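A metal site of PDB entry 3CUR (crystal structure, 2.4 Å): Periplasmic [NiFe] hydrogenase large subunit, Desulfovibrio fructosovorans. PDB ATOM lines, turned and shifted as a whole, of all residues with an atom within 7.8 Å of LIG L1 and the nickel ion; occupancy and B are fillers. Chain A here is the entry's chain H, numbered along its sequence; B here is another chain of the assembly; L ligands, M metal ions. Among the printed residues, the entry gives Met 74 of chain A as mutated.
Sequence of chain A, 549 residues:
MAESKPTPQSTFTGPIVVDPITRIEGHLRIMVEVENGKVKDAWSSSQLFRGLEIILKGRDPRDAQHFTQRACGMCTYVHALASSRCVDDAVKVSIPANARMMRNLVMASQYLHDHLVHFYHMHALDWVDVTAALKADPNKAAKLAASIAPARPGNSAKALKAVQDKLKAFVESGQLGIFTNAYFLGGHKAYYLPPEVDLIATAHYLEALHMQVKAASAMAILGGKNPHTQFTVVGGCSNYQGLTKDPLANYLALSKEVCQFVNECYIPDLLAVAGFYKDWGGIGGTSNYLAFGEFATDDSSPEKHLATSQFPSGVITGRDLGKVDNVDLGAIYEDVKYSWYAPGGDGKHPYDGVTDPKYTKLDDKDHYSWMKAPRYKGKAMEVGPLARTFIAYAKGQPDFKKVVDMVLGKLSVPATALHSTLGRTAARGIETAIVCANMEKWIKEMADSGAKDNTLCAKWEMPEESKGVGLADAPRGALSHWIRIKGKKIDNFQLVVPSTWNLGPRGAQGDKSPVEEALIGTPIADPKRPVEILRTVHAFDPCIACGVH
OG of Ser 499 lies within hydrogen-bond range of N of Cys 543, 2.9 Å away.
The side-chain carboxylate of Glu 25 sits close to the side-chain sulfur of Cys 543.
The side-chain sulfur (SG) of Cys 72 sits close to the backbone NH (N) of Met 74.
The side-chain sulfur (SG) of Cys 546 lies close to a ring nitrogen (NE2) of His 79 (3.2 Å).
The guanidinium group (NH2) of Arg 476 lies within hydrogen-bond range of the side-chain sulfur (SD) of Met 74 (3.2 Å).
The guanidinium group (NH2) of Arg 476 lies within salt-bridge range of the side-chain carboxylate (OD1) of Asp 114 (2.6 Å).
The guanidinium group (NH2) of Arg 476 is in salt-bridge range of the side-chain carboxylate (OD1) of Asp 541 (2.7 Å).
An oxygen (O1) of LIG L1 binds the nickel ion (1.9 Å).
SG of Cys 543 is bound to the nickel ion (2.2 Å).
The nickel ion is bound by the side-chain sulfur (SG) of Cys 72.
The side-chain sulfur (SG) of Cys 75 is bound to the nickel ion (2.4 Å).
The side-chain sulfur (SG) of Cys 546 binds the nickel ion (2.6 Å).
An oxygen (O1) of LIG L1 is bound to an iron atom (FE1) of LG2 L2 (1.9 Å).
Within 4 Å of LIG L1: Cys 72, Cys 75, Arg 476, Cys 543 and Cys 546.
The nearest printed residue that does not touch LIG L1 is Met 74 (4.2 Å).
NH1 of Arg 476 lies close to O2 of LIG L1.
An iron atom (FE1) of LG2 L2 is bound by the side-chain sulfur of Cys 75, 2.3 Å away.
The side-chain sulfur of Cys 546 binds an iron atom (FE1) of LG2 L2 (2.3 Å).
N2 of LG2 L2 is in hydrogen-bond range of N of Arg 476, 2.9 Å away.
The guanidinium group of Arg 476 lies close to a nitrogen (N2) of LG2 L2 (3.4 Å).
N of Ser 499 is in hydrogen-bond range of N1 of LG2 L2 (3.1 Å).
The side-chain hydroxyl of Ser 499 sits at hydrogen-bond distance from a nitrogen (N1) of LG2 L2 (2.7 Å).
A ring nitrogen (NE2) of His 79 is in hydrogen-bond range of an oxygen (O1) of LG2 L2, at 3.4 Å.
Of the 28 residues printed, 4 come within 4 Å of the nickel ion.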
ATOM      1  N   GLU A  25       9.595  17.162   8.576  1.00  0.00           N
ATOM      2  CA  GLU A  25      10.425  18.299   8.928  1.00  0.00           C
ATOM      3  C   GLU A  25      10.248  18.644  10.424  1.00  0.00           C
ATOM      4  O   GLU A  25       9.106  18.768  10.966  1.00  0.00           O
ATOM      5  CB  GLU A  25      10.092  19.494   8.025  1.00  0.00           C
ATOM      6  CG  GLU A  25      11.113  20.630   8.096  1.00  0.00           C
ATOM      7  CD  GLU A  25      11.237  21.184   9.500  1.00  0.00           C
ATOM      8  OE1 GLU A  25      10.187  21.480  10.118  1.00  0.00           O
ATOM      9  OE2 GLU A  25      12.389  21.339   9.994  1.00  0.00           O
ATOM     10  N   GLN A  69      11.047  33.058   5.281  1.00  0.00           N
ATOM     11  CA  GLN A  69      11.309  31.926   4.381  1.00  0.00           C
ATOM     12  C   GLN A  69      12.035  30.840   5.140  1.00  0.00           C
ATOM     13  O   GLN A  69      11.797  29.659   4.898  1.00  0.00           O
ATOM     14  CB  GLN A  69      12.078  32.297   3.118  1.00  0.00           C
ATOM     15  CG  GLN A  69      12.184  31.091   2.170  1.00  0.00           C
ATOM     16  CD  GLN A  69      12.663  31.413   0.782  1.00  0.00           C
ATOM     17  OE1 GLN A  69      12.361  30.679  -0.150  1.00  0.00           O
ATOM     18  NE2 GLN A  69      13.402  32.508   0.628  1.00  0.00           N
ATOM     19  N   ALA A  71      11.477  29.947   8.025  1.00  0.00           N
ATOM     20  CA  ALA A  71      10.593  29.164   8.871  1.00  0.00           C
ATOM     21  C   ALA A  71      10.748  27.684   8.505  1.00  0.00           C
ATOM     22  O   ALA A  71      10.623  26.793   9.349  1.00  0.00           O
ATOM     23  CB  ALA A  71       9.151  29.609   8.702  1.00  0.00           C
ATOM     24  N   CYS A  72      11.013  27.417   7.235  1.00  0.00           N
ATOM     25  CA  CYS A  72      11.108  26.056   6.775  1.00  0.00           C
ATOM     26  C   CYS A  72      11.768  26.014   5.429  1.00  0.00           C
ATOM     27  O   CYS A  72      11.451  26.817   4.572  1.00  0.00           O
ATOM     28  CB  CYS A  72       9.734  25.441   6.664  1.00  0.00           C
ATOM     29  SG  CYS A  72       9.892  23.689   6.388  1.00  0.00           S
ATOM     30  N   GLY A  73      12.667  25.048   5.265  1.00  0.00           N
ATOM     31  CA  GLY A  73      13.349  24.833   3.999  1.00  0.00           C
ATOM     32  C   GLY A  73      12.793  23.619   3.283  1.00  0.00           C
ATOM     33  O   GLY A  73      13.219  23.296   2.158  1.00  0.00           O
ATOM     34  N   MET A  74      11.873  22.902   3.915  1.00  0.00           N
ATOM     35  CA  MET A  74      11.207  21.845   3.198  1.00  0.00           C
ATOM     36  C   MET A  74      10.160  22.486   2.265  1.00  0.00           C
ATOM     37  O   MET A  74      10.246  22.343   1.034  1.00  0.00           O
ATOM     38  CB  MET A  74      10.633  20.768   4.115  1.00  0.00           C
ATOM     39  CG  MET A  74       9.945  19.664   3.296  1.00  0.00           C
ATOM     40  SD  MET A  74       9.504  18.228   4.273  1.00  0.00           S
ATOM     41  CE  MET A  74      11.151  17.678   4.712  1.00  0.00           C
ATOM     42  N   CYS A  75       9.211  23.207   2.849  1.00  0.00           N
ATOM     43  CA  CYS A  75       8.342  24.045   2.038  1.00  0.00           C
ATOM     44  C   CYS A  75       9.064  25.372   1.819  1.00  0.00           C
ATOM     45  O   CYS A  75       8.566  26.424   2.182  1.00  0.00           O
ATOM     46  CB  CYS A  75       6.968  24.260   2.717  1.00  0.00           C
ATOM     47  SG  CYS A  75       7.096  25.048   4.332  1.00  0.00           S
ATOM     48  N   THR A  76      10.239  25.330   1.208  1.00  0.00           N
ATOM     49  CA  THR A  76      10.944  26.578   0.886  1.00  0.00           C
ATOM     50  C   THR A  76      10.001  27.403  -0.009  1.00  0.00           C
ATOM     51  O   THR A  76       8.965  26.882  -0.458  1.00  0.00           O
ATOM     52  CB  THR A  76      12.286  26.289   0.163  1.00  0.00           C
ATOM     53  OG1 THR A  76      13.077  27.489   0.112  1.00  0.00           O
ATOM     54  CG2 THR A  76      12.032  25.775  -1.243  1.00  0.00           C
ATOM     55  N   VAL A  78       7.379  29.153   0.144  1.00  0.00           N
ATOM     56  CA  VAL A  78       5.971  29.519   0.458  1.00  0.00           C
ATOM     57  C   VAL A  78       5.855  30.704   1.432  1.00  0.00           C
ATOM     58  O   VAL A  78       5.035  31.569   1.239  1.00  0.00           O
ATOM     59  CB  VAL A  78       5.101  28.307   0.870  1.00  0.00           C
ATOM     60  CG1 VAL A  78       5.189  27.188  -0.233  1.00  0.00           C
ATOM     61  CG2 VAL A  78       5.512  27.768   2.245  1.00  0.00           C
ATOM     62  N   HIS A  79       6.707  30.742   2.461  1.00  0.00           N
ATOM     63  CA  HIS A  79       6.739  31.846   3.420  1.00  0.00           C
ATOM     64  C   HIS A  79       7.218  33.162   2.811  1.00  0.00           C
ATOM     65  O   HIS A  79       6.670  34.216   3.128  1.00  0.00           O
ATOM     66  CB  HIS A  79       7.580  31.483   4.632  1.00  0.00           C
ATOM     67  CG  HIS A  79       6.987  30.388   5.450  1.00  0.00           C
ATOM     68  ND1 HIS A  79       5.864  30.569   6.229  1.00  0.00           N
ATOM     69  CD2 HIS A  79       7.347  29.095   5.608  1.00  0.00           C
ATOM     70  CE1 HIS A  79       5.554  29.432   6.832  1.00  0.00           C
ATOM     71  NE2 HIS A  79       6.435  28.519   6.458  1.00  0.00           N
ATOM     72  N   GLN A 110       6.876  24.029  -6.485  1.00  0.00           N
ATOM     73  CA  GLN A 110       7.051  23.623  -5.086  1.00  0.00           C
ATOM     74  C   GLN A 110       6.138  22.465  -4.755  1.00  0.00           C
ATOM     75  O   GLN A 110       6.585  21.503  -4.130  1.00  0.00           O
ATOM     76  CB  GLN A 110       6.856  24.788  -4.103  1.00  0.00           C
ATOM     77  CG  GLN A 110       6.989  24.442  -2.629  1.00  0.00           C
ATOM     78  CD  GLN A 110       8.318  23.777  -2.212  1.00  0.00           C
ATOM     79  OE1 GLN A 110       9.360  23.951  -2.859  1.00  0.00           O
ATOM     80  NE2 GLN A 110       8.275  23.024  -1.119  1.00  0.00           N
ATOM     81  N   ASP A 114       7.663  18.944  -3.568  1.00  0.00           N
ATOM     82  CA  ASP A 114       7.330  18.673  -2.189  1.00  0.00           C
ATOM     83  C   ASP A 114       6.557  17.373  -2.075  1.00  0.00           C
ATOM     84  O   ASP A 114       6.931  16.516  -1.268  1.00  0.00           O
ATOM     85  CB  ASP A 114       6.524  19.838  -1.583  1.00  0.00           C
ATOM     86  CG  ASP A 114       6.715  19.967  -0.069  1.00  0.00           C
ATOM     87  OD1 ASP A 114       6.865  18.927   0.636  1.00  0.00           O
ATOM     88  OD2 ASP A 114       6.713  21.129   0.427  1.00  0.00           O
ATOM     89  N   ALA A 474      -0.079  26.554   0.745  1.00  0.00           N
ATOM     90  CA  ALA A 474       1.161  25.842   0.605  1.00  0.00           C
ATOM     91  C   ALA A 474       0.875  24.332   0.375  1.00  0.00           C
ATOM     92  O   ALA A 474      -0.270  23.876   0.491  1.00  0.00           O
ATOM     93  CB  ALA A 474       2.002  26.076   1.838  1.00  0.00           C
ATOM     94  N   PRO A 475       1.911  23.557   0.020  1.00  0.00           N
ATOM     95  CA  PRO A 475       1.723  22.104  -0.107  1.00  0.00           C
ATOM     96  C   PRO A 475       1.023  21.457   1.078  1.00  0.00           C
ATOM     97  O   PRO A 475       0.304  20.482   0.880  1.00  0.00           O
ATOM     98  CB  PRO A 475       3.137  21.579  -0.231  1.00  0.00           C
ATOM     99  CG  PRO A 475       3.877  22.763  -0.920  1.00  0.00           C
ATOM    100  CD  PRO A 475       3.288  23.978  -0.314  1.00  0.00           C
ATOM    101  N   ARG A 476       1.190  22.012   2.286  1.00  0.00           N
ATOM    102  CA  ARG A 476       0.561  21.454   3.495  1.00  0.00           C
ATOM    103  C   ARG A 476      -0.726  22.157   3.923  1.00  0.00           C
ATOM    104  O   ARG A 476      -1.398  21.731   4.867  1.00  0.00           O
ATOM    105  CB  ARG A 476       1.565  21.398   4.644  1.00  0.00           C
ATOM    106  CG  ARG A 476       2.615  20.301   4.463  1.00  0.00           C
ATOM    107  CD  ARG A 476       3.934  20.587   5.156  1.00  0.00           C
ATOM    108  NE  ARG A 476       4.940  19.611   4.709  1.00  0.00           N
ATOM    109  CZ  ARG A 476       5.679  19.758   3.613  1.00  0.00           C
ATOM    110  NH1 ARG A 476       5.560  20.838   2.856  1.00  0.00           N
ATOM    111  NH2 ARG A 476       6.540  18.825   3.263  1.00  0.00           N
ATOM    112  N   GLY A 477      -1.093  23.227   3.221  1.00  0.00           N
ATOM    113  CA  GLY A 477      -2.387  23.872   3.405  1.00  0.00           C
ATOM    114  C   GLY A 477      -2.345  25.363   3.670  1.00  0.00           C
ATOM    115  O   GLY A 477      -1.358  26.039   3.387  1.00  0.00           O
ATOM    116  N   VAL A 497       0.388  28.852  10.272  1.00  0.00           N
ATOM    117  CA  VAL A 497       0.974  27.956   9.287  1.00  0.00           C
ATOM    118  C   VAL A 497       0.203  26.638   9.265  1.00  0.00           C
ATOM    119  O   VAL A 497      -0.382  26.222  10.286  1.00  0.00           O
ATOM    120  CB  VAL A 497       2.511  27.783   9.549  1.00  0.00           C
ATOM    121  CG1 VAL A 497       3.220  27.055   8.409  1.00  0.00           C
ATOM    122  CG2 VAL A 497       3.173  29.136   9.688  1.00  0.00           C
ATOM    123  N   PRO A 498       0.129  25.995   8.089  1.00  0.00           N
ATOM    124  CA  PRO A 498      -0.721  24.812   7.937  1.00  0.00           C
ATOM    125  C   PRO A 498      -0.463  23.764   9.014  1.00  0.00           C
ATOM    126  O   PRO A 498      -1.413  23.211   9.553  1.00  0.00           O
ATOM    127  CB  PRO A 498      -0.304  24.248   6.579  1.00  0.00           C
ATOM    128  CG  PRO A 498       0.376  25.332   5.858  1.00  0.00           C
ATOM    129  CD  PRO A 498       0.795  26.380   6.828  1.00  0.00           C
ATOM    130  N   SER A 499       0.811  23.472   9.322  1.00  0.00           N
ATOM    131  CA  SER A 499       1.123  22.481  10.355  1.00  0.00           C
ATOM    132  C   SER A 499       0.670  22.969  11.719  1.00  0.00           C
ATOM    133  O   SER A 499       0.423  22.153  12.596  1.00  0.00           O
ATOM    134  CB  SER A 499       2.596  22.097  10.370  1.00  0.00           C
ATOM    135  OG  SER A 499       2.938  21.332   9.209  1.00  0.00           O
ATOM    136  N   ASP A 541       1.715  15.272   6.624  1.00  0.00           N
ATOM    137  CA  ASP A 541       2.944  15.885   6.103  1.00  0.00           C
ATOM    138  C   ASP A 541       3.420  16.988   7.051  1.00  0.00           C
ATOM    139  O   ASP A 541       3.506  18.156   6.678  1.00  0.00           O
ATOM    140  CB  ASP A 541       2.664  16.408   4.701  1.00  0.00           C
ATOM    141  CG  ASP A 541       3.907  16.857   3.948  1.00  0.00           C
ATOM    142  OD1 ASP A 541       5.054  16.867   4.485  1.00  0.00           O
ATOM    143  OD2 ASP A 541       3.691  17.239   2.764  1.00  0.00           O
ATOM    144  N   PRO A 542       3.723  16.626   8.311  1.00  0.00           N
ATOM    145  CA  PRO A 542       4.036  17.615   9.322  1.00  0.00           C
ATOM    146  C   PRO A 542       5.319  18.370   9.042  1.00  0.00           C
ATOM    147  O   PRO A 542       6.282  17.805   8.501  1.00  0.00           O
ATOM    148  CB  PRO A 542       4.246  16.779  10.594  1.00  0.00           C
ATOM    149  CG  PRO A 542       3.560  15.512  10.328  1.00  0.00           C
ATOM    150  CD  PRO A 542       3.777  15.260   8.858  1.00  0.00           C
ATOM    151  N   CYS A 543       5.309  19.647   9.406  1.00  0.00           N
ATOM    152  CA  CYS A 543       6.472  20.518   9.369  1.00  0.00           C
ATOM    153  C   CYS A 543       6.487  21.320  10.672  1.00  0.00           C
ATOM    154  O   CYS A 543       5.738  22.295  10.826  1.00  0.00           O
ATOM    155  CB  CYS A 543       6.406  21.439   8.162  1.00  0.00           C
ATOM    156  SG  CYS A 543       7.965  22.223   7.804  1.00  0.00           S
ATOM    157  N   ILE A 544       7.353  20.918  11.608  1.00  0.00           N
ATOM    158  CA  ILE A 544       7.304  21.503  12.934  1.00  0.00           C
ATOM    159  C   ILE A 544       7.973  22.878  12.942  1.00  0.00           C
ATOM    160  O   ILE A 544       7.592  23.766  13.703  1.00  0.00           O
ATOM    161  CB  ILE A 544       7.850  20.546  14.013  1.00  0.00           C
ATOM    162  CG1 ILE A 544       7.191  19.148  13.914  1.00  0.00           C
ATOM    163  CG2 ILE A 544       7.671  21.122  15.427  1.00  0.00           C
ATOM    164  CD1 ILE A 544       5.660  19.107  13.653  1.00  0.00           C
ATOM    165  N   ALA A 545       8.962  23.050  12.062  1.00  0.00           N
ATOM    166  CA  ALA A 545       9.648  24.335  11.913  1.00  0.00           C
ATOM    167  C   ALA A 545       8.640  25.359  11.385  1.00  0.00           C
ATOM    168  O   ALA A 545       8.600  26.508  11.859  1.00  0.00           O
ATOM    169  CB  ALA A 545      10.849  24.187  10.982  1.00  0.00           C
ATOM    170  N   CYS A 546       7.815  24.925  10.437  1.00  0.00           N
ATOM    171  CA  CYS A 546       6.671  25.679   9.972  1.00  0.00           C
ATOM    172  C   CYS A 546       5.669  25.933  11.088  1.00  0.00           C
ATOM    173  O   CYS A 546       5.235  27.061  11.297  1.00  0.00           O
ATOM    174  CB  CYS A 546       5.946  24.899   8.868  1.00  0.00           C
ATOM    175  SG  CYS A 546       6.377  25.365   7.203  1.00  0.00           S
ATOM    176  N   GLY A 547       5.281  24.869  11.788  1.00  0.00           N
ATOM    177  CA  GLY A 547       4.204  24.977  12.742  1.00  0.00           C
ATOM    178  C   GLY A 547       4.496  25.949  13.860  1.00  0.00           C
ATOM    179  O   GLY A 547       3.614  26.708  14.257  1.00  0.00           O
ATOM    180  N   CYS B  17      15.809  24.626   9.856  1.00  0.00           N
ATOM    181  CA  CYS B  17      14.610  24.701   9.018  1.00  0.00           C
ATOM    182  C   CYS B  17      14.616  23.578   7.985  1.00  0.00           C
ATOM    183  O   CYS B  17      13.691  23.437   7.201  1.00  0.00           O
ATOM    184  CB  CYS B  17      14.568  26.060   8.308  1.00  0.00           C
ATOM    185  SG  CYS B  17      15.563  26.086   6.808  1.00  0.00           S
ATOM    186  N   THR B  18      15.707  22.795   7.966  1.00  0.00           N
ATOM    187  CA  THR B  18      15.855  21.592   7.135  1.00  0.00           C
ATOM    188  C   THR B  18      16.231  21.935   5.678  1.00  0.00           C
ATOM    189  O   THR B  18      16.317  21.049   4.804  1.00  0.00           O
ATOM    190  CB  THR B  18      14.600  20.675   7.249  1.00  0.00           C
ATOM    191  OG1 THR B  18      14.312  20.437   8.642  1.00  0.00           O
ATOM    192  CG2 THR B  18      14.811  19.342   6.531  1.00  0.00           C
HETATM  193  O1  LIG L   1       5.904  22.904   5.791  1.00  0.00           O
HETATM  194  O2  LIG L   1       6.645  21.927   5.001  1.00  0.00           O
HETATM  195 FE1  LG2 L   2       5.184  24.622   5.441  1.00  0.00          FE
HETATM  196  C1  LG2 L   2       3.967  23.880   6.696  1.00  0.00           C
HETATM  197  N1  LG2 L   2       3.234  23.418   7.456  1.00  0.00           N
HETATM  198  C2  LG2 L   2       4.136  23.898   4.012  1.00  0.00           C
HETATM  199  N2  LG2 L   2       3.505  23.586   3.082  1.00  0.00           N
HETATM  200  C3  LG2 L   2       4.252  26.052   5.236  1.00  0.00           C
HETATM  201  O1  LG2 L   2       3.696  27.052   5.040  1.00  0.00           O
HETATM  202 NI    NI M   1       7.684  23.511   6.026  1.00  0.00          NI
